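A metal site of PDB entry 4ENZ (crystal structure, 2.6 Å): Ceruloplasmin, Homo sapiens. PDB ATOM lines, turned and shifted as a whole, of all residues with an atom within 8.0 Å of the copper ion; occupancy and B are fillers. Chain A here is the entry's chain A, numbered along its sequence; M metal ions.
ND1 of His 704 is bound to the copper ion, at 1.9 Å.
The copper ion is bound by ND1 of His 656, 2.0 Å away.
The side-chain sulfur (SG) of Cys 699 is bound to the copper ion (2.2 Å).
SD of Met 709 is bound to the copper ion, 2.8 Å away.
The copper ion has four donor atoms within binding distance.
Thr 701 touches the copper ion.
Five residues have an atom within 4 Å of the copper ion: His 656, Cys 699, Thr 701, His 704 and Met 709.
NE2 of His 704 lies within hydrogen-bond range of OE2 of Glu 990 (3.4 Å).
NE2 of His 704 lies within hydrogen-bond range of O of Ala 653 (2.9 Å).
The side-chain hydroxyl (OG) of Ser 648 sits at hydrogen-bond distance from a ring nitrogen (NE2) of His 656 (3.4 Å).
The side-chain sulfur (SG) of Cys 699 lies close to the side-chain hydroxyl (OG1) of Thr 701 (2.9 Å).
The backbone NH (N) of Gly 657 lies close to the side-chain sulfur (SG) of Cys 699, 3.4 Å away.
OD1 of Asp 654 sits at hydrogen-bond distance from NE2 of His 656, 3.2 Å away.
The backbone carbonyl oxygen (O) of Leu 677 lies within hydrogen-bond range of the backbone NH (N) of His 656 (2.9 Å).
A ring nitrogen (ND1) of His 704 lies close to the side-chain hydroxyl of Thr 701, 2.6 Å away.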
ATOM      1  N   PRO A 582      -8.849 -19.086  22.806  1.00  0.00           N
ATOM      2  CA  PRO A 582      -9.035 -19.719  24.058  1.00  0.00           C
ATOM      3  C   PRO A 582      -8.007 -19.224  25.054  1.00  0.00           C
ATOM      4  O   PRO A 582      -6.799 -19.073  24.709  1.00  0.00           O
ATOM      5  CB  PRO A 582      -8.751 -21.184  23.739  1.00  0.00           C
ATOM      6  CG  PRO A 582      -7.708 -21.128  22.670  1.00  0.00           C
ATOM      7  CD  PRO A 582      -7.889 -19.807  21.957  1.00  0.00           C
ATOM      8  N   THR A 583      -8.460 -18.974  26.275  1.00  0.00           N
ATOM      9  CA  THR A 583      -7.553 -18.616  27.333  1.00  0.00           C
ATOM     10  C   THR A 583      -8.218 -18.759  28.677  1.00  0.00           C
ATOM     11  O   THR A 583      -9.431 -18.971  28.759  1.00  0.00           O
ATOM     12  CB  THR A 583      -7.089 -17.173  27.207  1.00  0.00           C
ATOM     13  OG1 THR A 583      -6.182 -16.880  28.281  1.00  0.00           O
ATOM     14  CG2 THR A 583      -8.285 -16.214  27.264  1.00  0.00           C
ATOM     15  N   VAL A 584      -7.422 -18.661  29.728  1.00  0.00           N
ATOM     16  CA  VAL A 584      -7.953 -18.574  31.066  1.00  0.00           C
ATOM     17  C   VAL A 584      -8.054 -17.090  31.397  1.00  0.00           C
ATOM     18  O   VAL A 584      -7.007 -16.413  31.575  1.00  0.00           O
ATOM     19  CB  VAL A 584      -7.055 -19.283  32.071  1.00  0.00           C
ATOM     20  CG1 VAL A 584      -7.718 -19.315  33.410  1.00  0.00           C
ATOM     21  CG2 VAL A 584      -6.711 -20.673  31.607  1.00  0.00           C
ATOM     22  N   HIS A 621     -12.188 -20.105  32.246  1.00  0.00           N
ATOM     23  CA  HIS A 621     -11.670 -20.898  31.166  1.00  0.00           C
ATOM     24  C   HIS A 621     -12.633 -20.871  30.022  1.00  0.00           C
ATOM     25  O   HIS A 621     -13.727 -21.441  30.118  1.00  0.00           O
ATOM     26  CB  HIS A 621     -11.549 -22.345  31.619  1.00  0.00           C
ATOM     27  CG  HIS A 621     -10.493 -22.579  32.666  1.00  0.00           C
ATOM     28  ND1 HIS A 621     -10.698 -22.289  33.991  1.00  0.00           N
ATOM     29  CD2 HIS A 621      -9.248 -23.092  32.570  1.00  0.00           C
ATOM     30  CE1 HIS A 621      -9.616 -22.615  34.668  1.00  0.00           C
ATOM     31  NE2 HIS A 621      -8.714 -23.115  33.833  1.00  0.00           N
ATOM     32  N   SER A 622     -12.209 -20.292  28.904  1.00  0.00           N
ATOM     33  CA  SER A 622     -13.159 -19.818  27.928  1.00  0.00           C
ATOM     34  C   SER A 622     -12.589 -19.735  26.513  1.00  0.00           C
ATOM     35  O   SER A 622     -11.390 -19.759  26.340  1.00  0.00           O
ATOM     36  CB  SER A 622     -13.664 -18.427  28.393  1.00  0.00           C
ATOM     37  OG  SER A 622     -12.597 -17.478  28.501  1.00  0.00           O
ATOM     38  N   MET A 623     -13.501 -19.644  25.533  1.00  0.00           N
ATOM     39  CA  MET A 623     -13.192 -19.397  24.120  1.00  0.00           C
ATOM     40  C   MET A 623     -13.946 -18.109  23.701  1.00  0.00           C
ATOM     41  O   MET A 623     -15.178 -18.040  23.796  1.00  0.00           O
ATOM     42  CB  MET A 623     -13.654 -20.565  23.232  1.00  0.00           C
ATOM     43  CG  MET A 623     -12.564 -21.448  22.637  1.00  0.00           C
ATOM     44  SD  MET A 623     -12.840 -23.270  22.867  1.00  0.00           S
ATOM     45  CE  MET A 623     -13.026 -23.453  24.634  1.00  0.00           C
ATOM     46  N   SER A 648      -3.687 -17.503  21.320  1.00  0.00           N
ATOM     47  CA  SER A 648      -3.898 -17.431  22.755  1.00  0.00           C
ATOM     48  C   SER A 648      -2.929 -16.453  23.396  1.00  0.00           C
ATOM     49  O   SER A 648      -1.991 -15.989  22.781  1.00  0.00           O
ATOM     50  CB  SER A 648      -3.738 -18.821  23.400  1.00  0.00           C
ATOM     51  OG  SER A 648      -4.095 -18.792  24.781  1.00  0.00           O
ATOM     52  N   ALA A 653      -0.304 -21.587  32.740  1.00  0.00           N
ATOM     53  CA  ALA A 653      -1.546 -22.378  32.744  1.00  0.00           C
ATOM     54  C   ALA A 653      -2.106 -22.545  31.324  1.00  0.00           C
ATOM     55  O   ALA A 653      -2.950 -23.403  31.071  1.00  0.00           O
ATOM     56  CB  ALA A 653      -2.592 -21.729  33.670  1.00  0.00           C
ATOM     57  N   ASP A 654      -1.632 -21.702  30.409  1.00  0.00           N
ATOM     58  CA  ASP A 654      -2.176 -21.654  29.063  1.00  0.00           C
ATOM     59  C   ASP A 654      -1.430 -22.576  28.119  1.00  0.00           C
ATOM     60  O   ASP A 654      -0.712 -22.125  27.241  1.00  0.00           O
ATOM     61  CB  ASP A 654      -2.158 -20.219  28.547  1.00  0.00           C
ATOM     62  CG  ASP A 654      -3.151 -19.330  29.309  1.00  0.00           C
ATOM     63  OD1 ASP A 654      -4.363 -19.387  28.960  1.00  0.00           O
ATOM     64  OD2 ASP A 654      -2.735 -18.591  30.235  1.00  0.00           O
ATOM     65  N   VAL A 655      -1.594 -23.885  28.330  1.00  0.00           N
ATOM     66  CA  VAL A 655      -1.144 -24.877  27.371  1.00  0.00           C
ATOM     67  C   VAL A 655      -2.405 -25.601  26.903  1.00  0.00           C
ATOM     68  O   VAL A 655      -3.128 -26.220  27.695  1.00  0.00           O
ATOM     69  CB  VAL A 655      -0.062 -25.847  27.931  1.00  0.00           C
ATOM     70  CG1 VAL A 655       0.668 -25.215  29.112  1.00  0.00           C
ATOM     71  CG2 VAL A 655      -0.646 -27.205  28.277  1.00  0.00           C
ATOM     72  N   HIS A 656      -2.701 -25.441  25.612  1.00  0.00           N
ATOM     73  CA  HIS A 656      -4.036 -25.695  25.133  1.00  0.00           C
ATOM     74  C   HIS A 656      -3.879 -26.698  24.057  1.00  0.00           C
ATOM     75  O   HIS A 656      -2.868 -26.631  23.346  1.00  0.00           O
ATOM     76  CB  HIS A 656      -4.642 -24.449  24.517  1.00  0.00           C
ATOM     77  CG  HIS A 656      -4.913 -23.350  25.488  1.00  0.00           C
ATOM     78  ND1 HIS A 656      -5.939 -23.407  26.397  1.00  0.00           N
ATOM     79  CD2 HIS A 656      -4.304 -22.156  25.662  1.00  0.00           C
ATOM     80  CE1 HIS A 656      -5.940 -22.291  27.117  1.00  0.00           C
ATOM     81  NE2 HIS A 656      -4.967 -21.512  26.684  1.00  0.00           N
ATOM     82  N   GLY A 657      -4.852 -27.598  23.941  1.00  0.00           N
ATOM     83  CA  GLY A 657      -4.954 -28.515  22.817  1.00  0.00           C
ATOM     84  C   GLY A 657      -6.362 -28.456  22.226  1.00  0.00           C
ATOM     85  O   GLY A 657      -7.214 -29.219  22.650  1.00  0.00           O
ATOM     86  N   ILE A 658      -6.593 -27.569  21.251  1.00  0.00           N
ATOM     87  CA  ILE A 658      -7.908 -27.287  20.740  1.00  0.00           C
ATOM     88  C   ILE A 658      -8.285 -28.345  19.735  1.00  0.00           C
ATOM     89  O   ILE A 658      -7.754 -28.387  18.644  1.00  0.00           O
ATOM     90  CB  ILE A 658      -7.971 -25.907  20.080  1.00  0.00           C
ATOM     91  CG1 ILE A 658      -7.470 -24.837  21.047  1.00  0.00           C
ATOM     92  CG2 ILE A 658      -9.385 -25.574  19.645  1.00  0.00           C
ATOM     93  CD1 ILE A 658      -8.132 -24.899  22.390  1.00  0.00           C
ATOM     94  N   ALA A 675      -5.084 -28.584  17.851  1.00  0.00           N
ATOM     95  CA  ALA A 675      -4.115 -27.492  17.678  1.00  0.00           C
ATOM     96  C   ALA A 675      -3.497 -27.115  19.009  1.00  0.00           C
ATOM     97  O   ALA A 675      -4.233 -26.824  19.951  1.00  0.00           O
ATOM     98  CB  ALA A 675      -4.813 -26.314  17.097  1.00  0.00           C
ATOM     99  N   LEU A 677      -1.580 -24.571  21.609  1.00  0.00           N
ATOM    100  CA  LEU A 677      -1.431 -23.124  21.757  1.00  0.00           C
ATOM    101  C   LEU A 677      -0.915 -22.733  23.118  1.00  0.00           C
ATOM    102  O   LEU A 677      -1.207 -23.394  24.125  1.00  0.00           O
ATOM    103  CB  LEU A 677      -2.759 -22.434  21.565  1.00  0.00           C
ATOM    104  CG  LEU A 677      -3.260 -22.419  20.117  1.00  0.00           C
ATOM    105  CD1 LEU A 677      -4.706 -22.060  20.163  1.00  0.00           C
ATOM    106  CD2 LEU A 677      -2.494 -21.414  19.319  1.00  0.00           C
ATOM    107  N   GLU A 698     -13.179 -28.074  21.490  1.00  0.00           N
ATOM    108  CA  GLU A 698     -12.946 -28.081  22.919  1.00  0.00           C
ATOM    109  C   GLU A 698     -11.478 -28.193  23.202  1.00  0.00           C
ATOM    110  O   GLU A 698     -10.727 -28.711  22.373  1.00  0.00           O
ATOM    111  CB  GLU A 698     -13.661 -29.269  23.521  1.00  0.00           C
ATOM    112  CG  GLU A 698     -12.981 -30.602  23.180  1.00  0.00           C
ATOM    113  CD  GLU A 698     -13.860 -31.825  23.486  1.00  0.00           C
ATOM    114  OE1 GLU A 698     -15.095 -31.711  23.450  1.00  0.00           O
ATOM    115  OE2 GLU A 698     -13.280 -32.901  23.742  1.00  0.00           O
ATOM    116  N   CYS A 699     -11.062 -27.730  24.376  1.00  0.00           N
ATOM    117  CA  CYS A 699      -9.684 -27.955  24.826  1.00  0.00           C
ATOM    118  C   CYS A 699      -9.527 -29.334  25.480  1.00  0.00           C
ATOM    119  O   CYS A 699     -10.249 -29.676  26.390  1.00  0.00           O
ATOM    120  CB  CYS A 699      -9.204 -26.858  25.776  1.00  0.00           C
ATOM    121  SG  CYS A 699      -7.421 -26.939  26.010  1.00  0.00           S
ATOM    122  N   LEU A 700      -8.616 -30.114  24.948  1.00  0.00           N
ATOM    123  CA  LEU A 700      -8.285 -31.433  25.475  1.00  0.00           C
ATOM    124  C   LEU A 700      -7.686 -31.375  26.894  1.00  0.00           C
ATOM    125  O   LEU A 700      -7.826 -32.338  27.657  1.00  0.00           O
ATOM    126  CB  LEU A 700      -7.240 -32.117  24.560  1.00  0.00           C
ATOM    127  CG  LEU A 700      -7.858 -33.067  23.564  1.00  0.00           C
ATOM    128  CD1 LEU A 700      -6.851 -33.516  22.518  1.00  0.00           C
ATOM    129  CD2 LEU A 700      -8.415 -34.246  24.352  1.00  0.00           C
ATOM    130  N   THR A 701      -6.974 -30.286  27.216  1.00  0.00           N
ATOM    131  CA  THR A 701      -6.257 -30.196  28.485  1.00  0.00           C
ATOM    132  C   THR A 701      -7.268 -30.306  29.608  1.00  0.00           C
ATOM    133  O   THR A 701      -8.248 -29.584  29.692  1.00  0.00           O
ATOM    134  CB  THR A 701      -5.429 -28.914  28.621  1.00  0.00           C
ATOM    135  OG1 THR A 701      -6.349 -27.833  28.586  1.00  0.00           O
ATOM    136  CG2 THR A 701      -4.500 -28.733  27.458  1.00  0.00           C
ATOM    137  N   THR A 702      -7.003 -31.264  30.472  1.00  0.00           N
ATOM    138  CA  THR A 702      -7.971 -31.776  31.438  1.00  0.00           C
ATOM    139  C   THR A 702      -8.721 -30.732  32.243  1.00  0.00           C
ATOM    140  O   THR A 702      -9.969 -30.700  32.230  1.00  0.00           O
ATOM    141  CB  THR A 702      -7.241 -32.813  32.264  1.00  0.00           C
ATOM    142  OG1 THR A 702      -7.525 -34.073  31.629  1.00  0.00           O
ATOM    143  CG2 THR A 702      -7.607 -32.770  33.790  1.00  0.00           C
ATOM    144  N   ASP A 703      -7.977 -29.847  32.914  1.00  0.00           N
ATOM    145  CA  ASP A 703      -8.627 -28.807  33.698  1.00  0.00           C
ATOM    146  C   ASP A 703      -9.344 -27.754  32.864  1.00  0.00           C
ATOM    147  O   ASP A 703     -10.381 -27.233  33.311  1.00  0.00           O
ATOM    148  CB  ASP A 703      -7.646 -28.141  34.660  1.00  0.00           C
ATOM    149  CG  ASP A 703      -7.296 -29.048  35.875  1.00  0.00           C
ATOM    150  OD1 ASP A 703      -7.981 -30.106  36.097  1.00  0.00           O
ATOM    151  OD2 ASP A 703      -6.326 -28.700  36.593  1.00  0.00           O
ATOM    152  N   HIS A 704      -8.836 -27.458  31.665  1.00  0.00           N
ATOM    153  CA  HIS A 704      -9.547 -26.503  30.821  1.00  0.00           C
ATOM    154  C   HIS A 704     -10.922 -27.059  30.449  1.00  0.00           C
ATOM    155  O   HIS A 704     -11.921 -26.359  30.477  1.00  0.00           O
ATOM    156  CB  HIS A 704      -8.764 -26.112  29.562  1.00  0.00           C
ATOM    157  CG  HIS A 704      -7.398 -25.553  29.821  1.00  0.00           C
ATOM    158  ND1 HIS A 704      -6.530 -25.219  28.810  1.00  0.00           N
ATOM    159  CD2 HIS A 704      -6.739 -25.302  30.984  1.00  0.00           C
ATOM    160  CE1 HIS A 704      -5.399 -24.764  29.336  1.00  0.00           C
ATOM    161  NE2 HIS A 704      -5.503 -24.817  30.651  1.00  0.00           N
ATOM    162  N   TYR A 705     -10.988 -28.347  30.168  1.00  0.00           N
ATOM    163  CA  TYR A 705     -12.256 -28.941  29.763  1.00  0.00           C
ATOM    164  C   TYR A 705     -13.249 -28.924  30.946  1.00  0.00           C
ATOM    165  O   TYR A 705     -14.334 -28.379  30.842  1.00  0.00           O
ATOM    166  CB  TYR A 705     -12.030 -30.363  29.198  1.00  0.00           C
ATOM    167  CG  TYR A 705     -13.304 -31.010  28.732  1.00  0.00           C
ATOM    168  CD1 TYR A 705     -13.804 -30.774  27.441  1.00  0.00           C
ATOM    169  CD2 TYR A 705     -14.041 -31.795  29.575  1.00  0.00           C
ATOM    170  CE1 TYR A 705     -15.013 -31.337  26.994  1.00  0.00           C
ATOM    171  CE2 TYR A 705     -15.257 -32.398  29.133  1.00  0.00           C
ATOM    172  CZ  TYR A 705     -15.742 -32.146  27.849  1.00  0.00           C
ATOM    173  OH  TYR A 705     -16.918 -32.745  27.445  1.00  0.00           O
ATOM    174  N   MET A 709     -13.970 -24.975  28.981  1.00  0.00           N
ATOM    175  CA  MET A 709     -13.377 -24.550  27.709  1.00  0.00           C
ATOM    176  C   MET A 709     -13.852 -25.523  26.655  1.00  0.00           C
ATOM    177  O   MET A 709     -13.105 -26.354  26.206  1.00  0.00           O
ATOM    178  CB  MET A 709     -11.836 -24.498  27.789  1.00  0.00           C
ATOM    179  CG  MET A 709     -11.090 -23.568  26.778  1.00  0.00           C
ATOM    180  SD  MET A 709      -9.238 -23.541  26.955  1.00  0.00           S
ATOM    181  CE  MET A 709      -9.179 -22.534  28.495  1.00  0.00           C
ATOM    182  N   GLU A 990      -2.542 -29.089  32.282  1.00  0.00           N
ATOM    183  CA  GLU A 990      -1.621 -27.927  32.100  1.00  0.00           C
ATOM    184  C   GLU A 990      -0.158 -28.331  32.249  1.00  0.00           C
ATOM    185  O   GLU A 990       0.716 -27.870  31.543  1.00  0.00           O
ATOM    186  CB  GLU A 990      -1.934 -26.853  33.169  1.00  0.00           C
ATOM    187  CG  GLU A 990      -3.322 -26.223  33.008  1.00  0.00           C
ATOM    188  CD  GLU A 990      -3.750 -25.282  34.146  1.00  0.00           C
ATOM    189  OE1 GLU A 990      -3.090 -25.234  35.211  1.00  0.00           O
ATOM    190  OE2 GLU A 990      -4.785 -24.577  33.935  1.00  0.00           O
HETATM  191 CU    CU M   1      -6.913 -25.047  26.965  1.00  0.00          CU
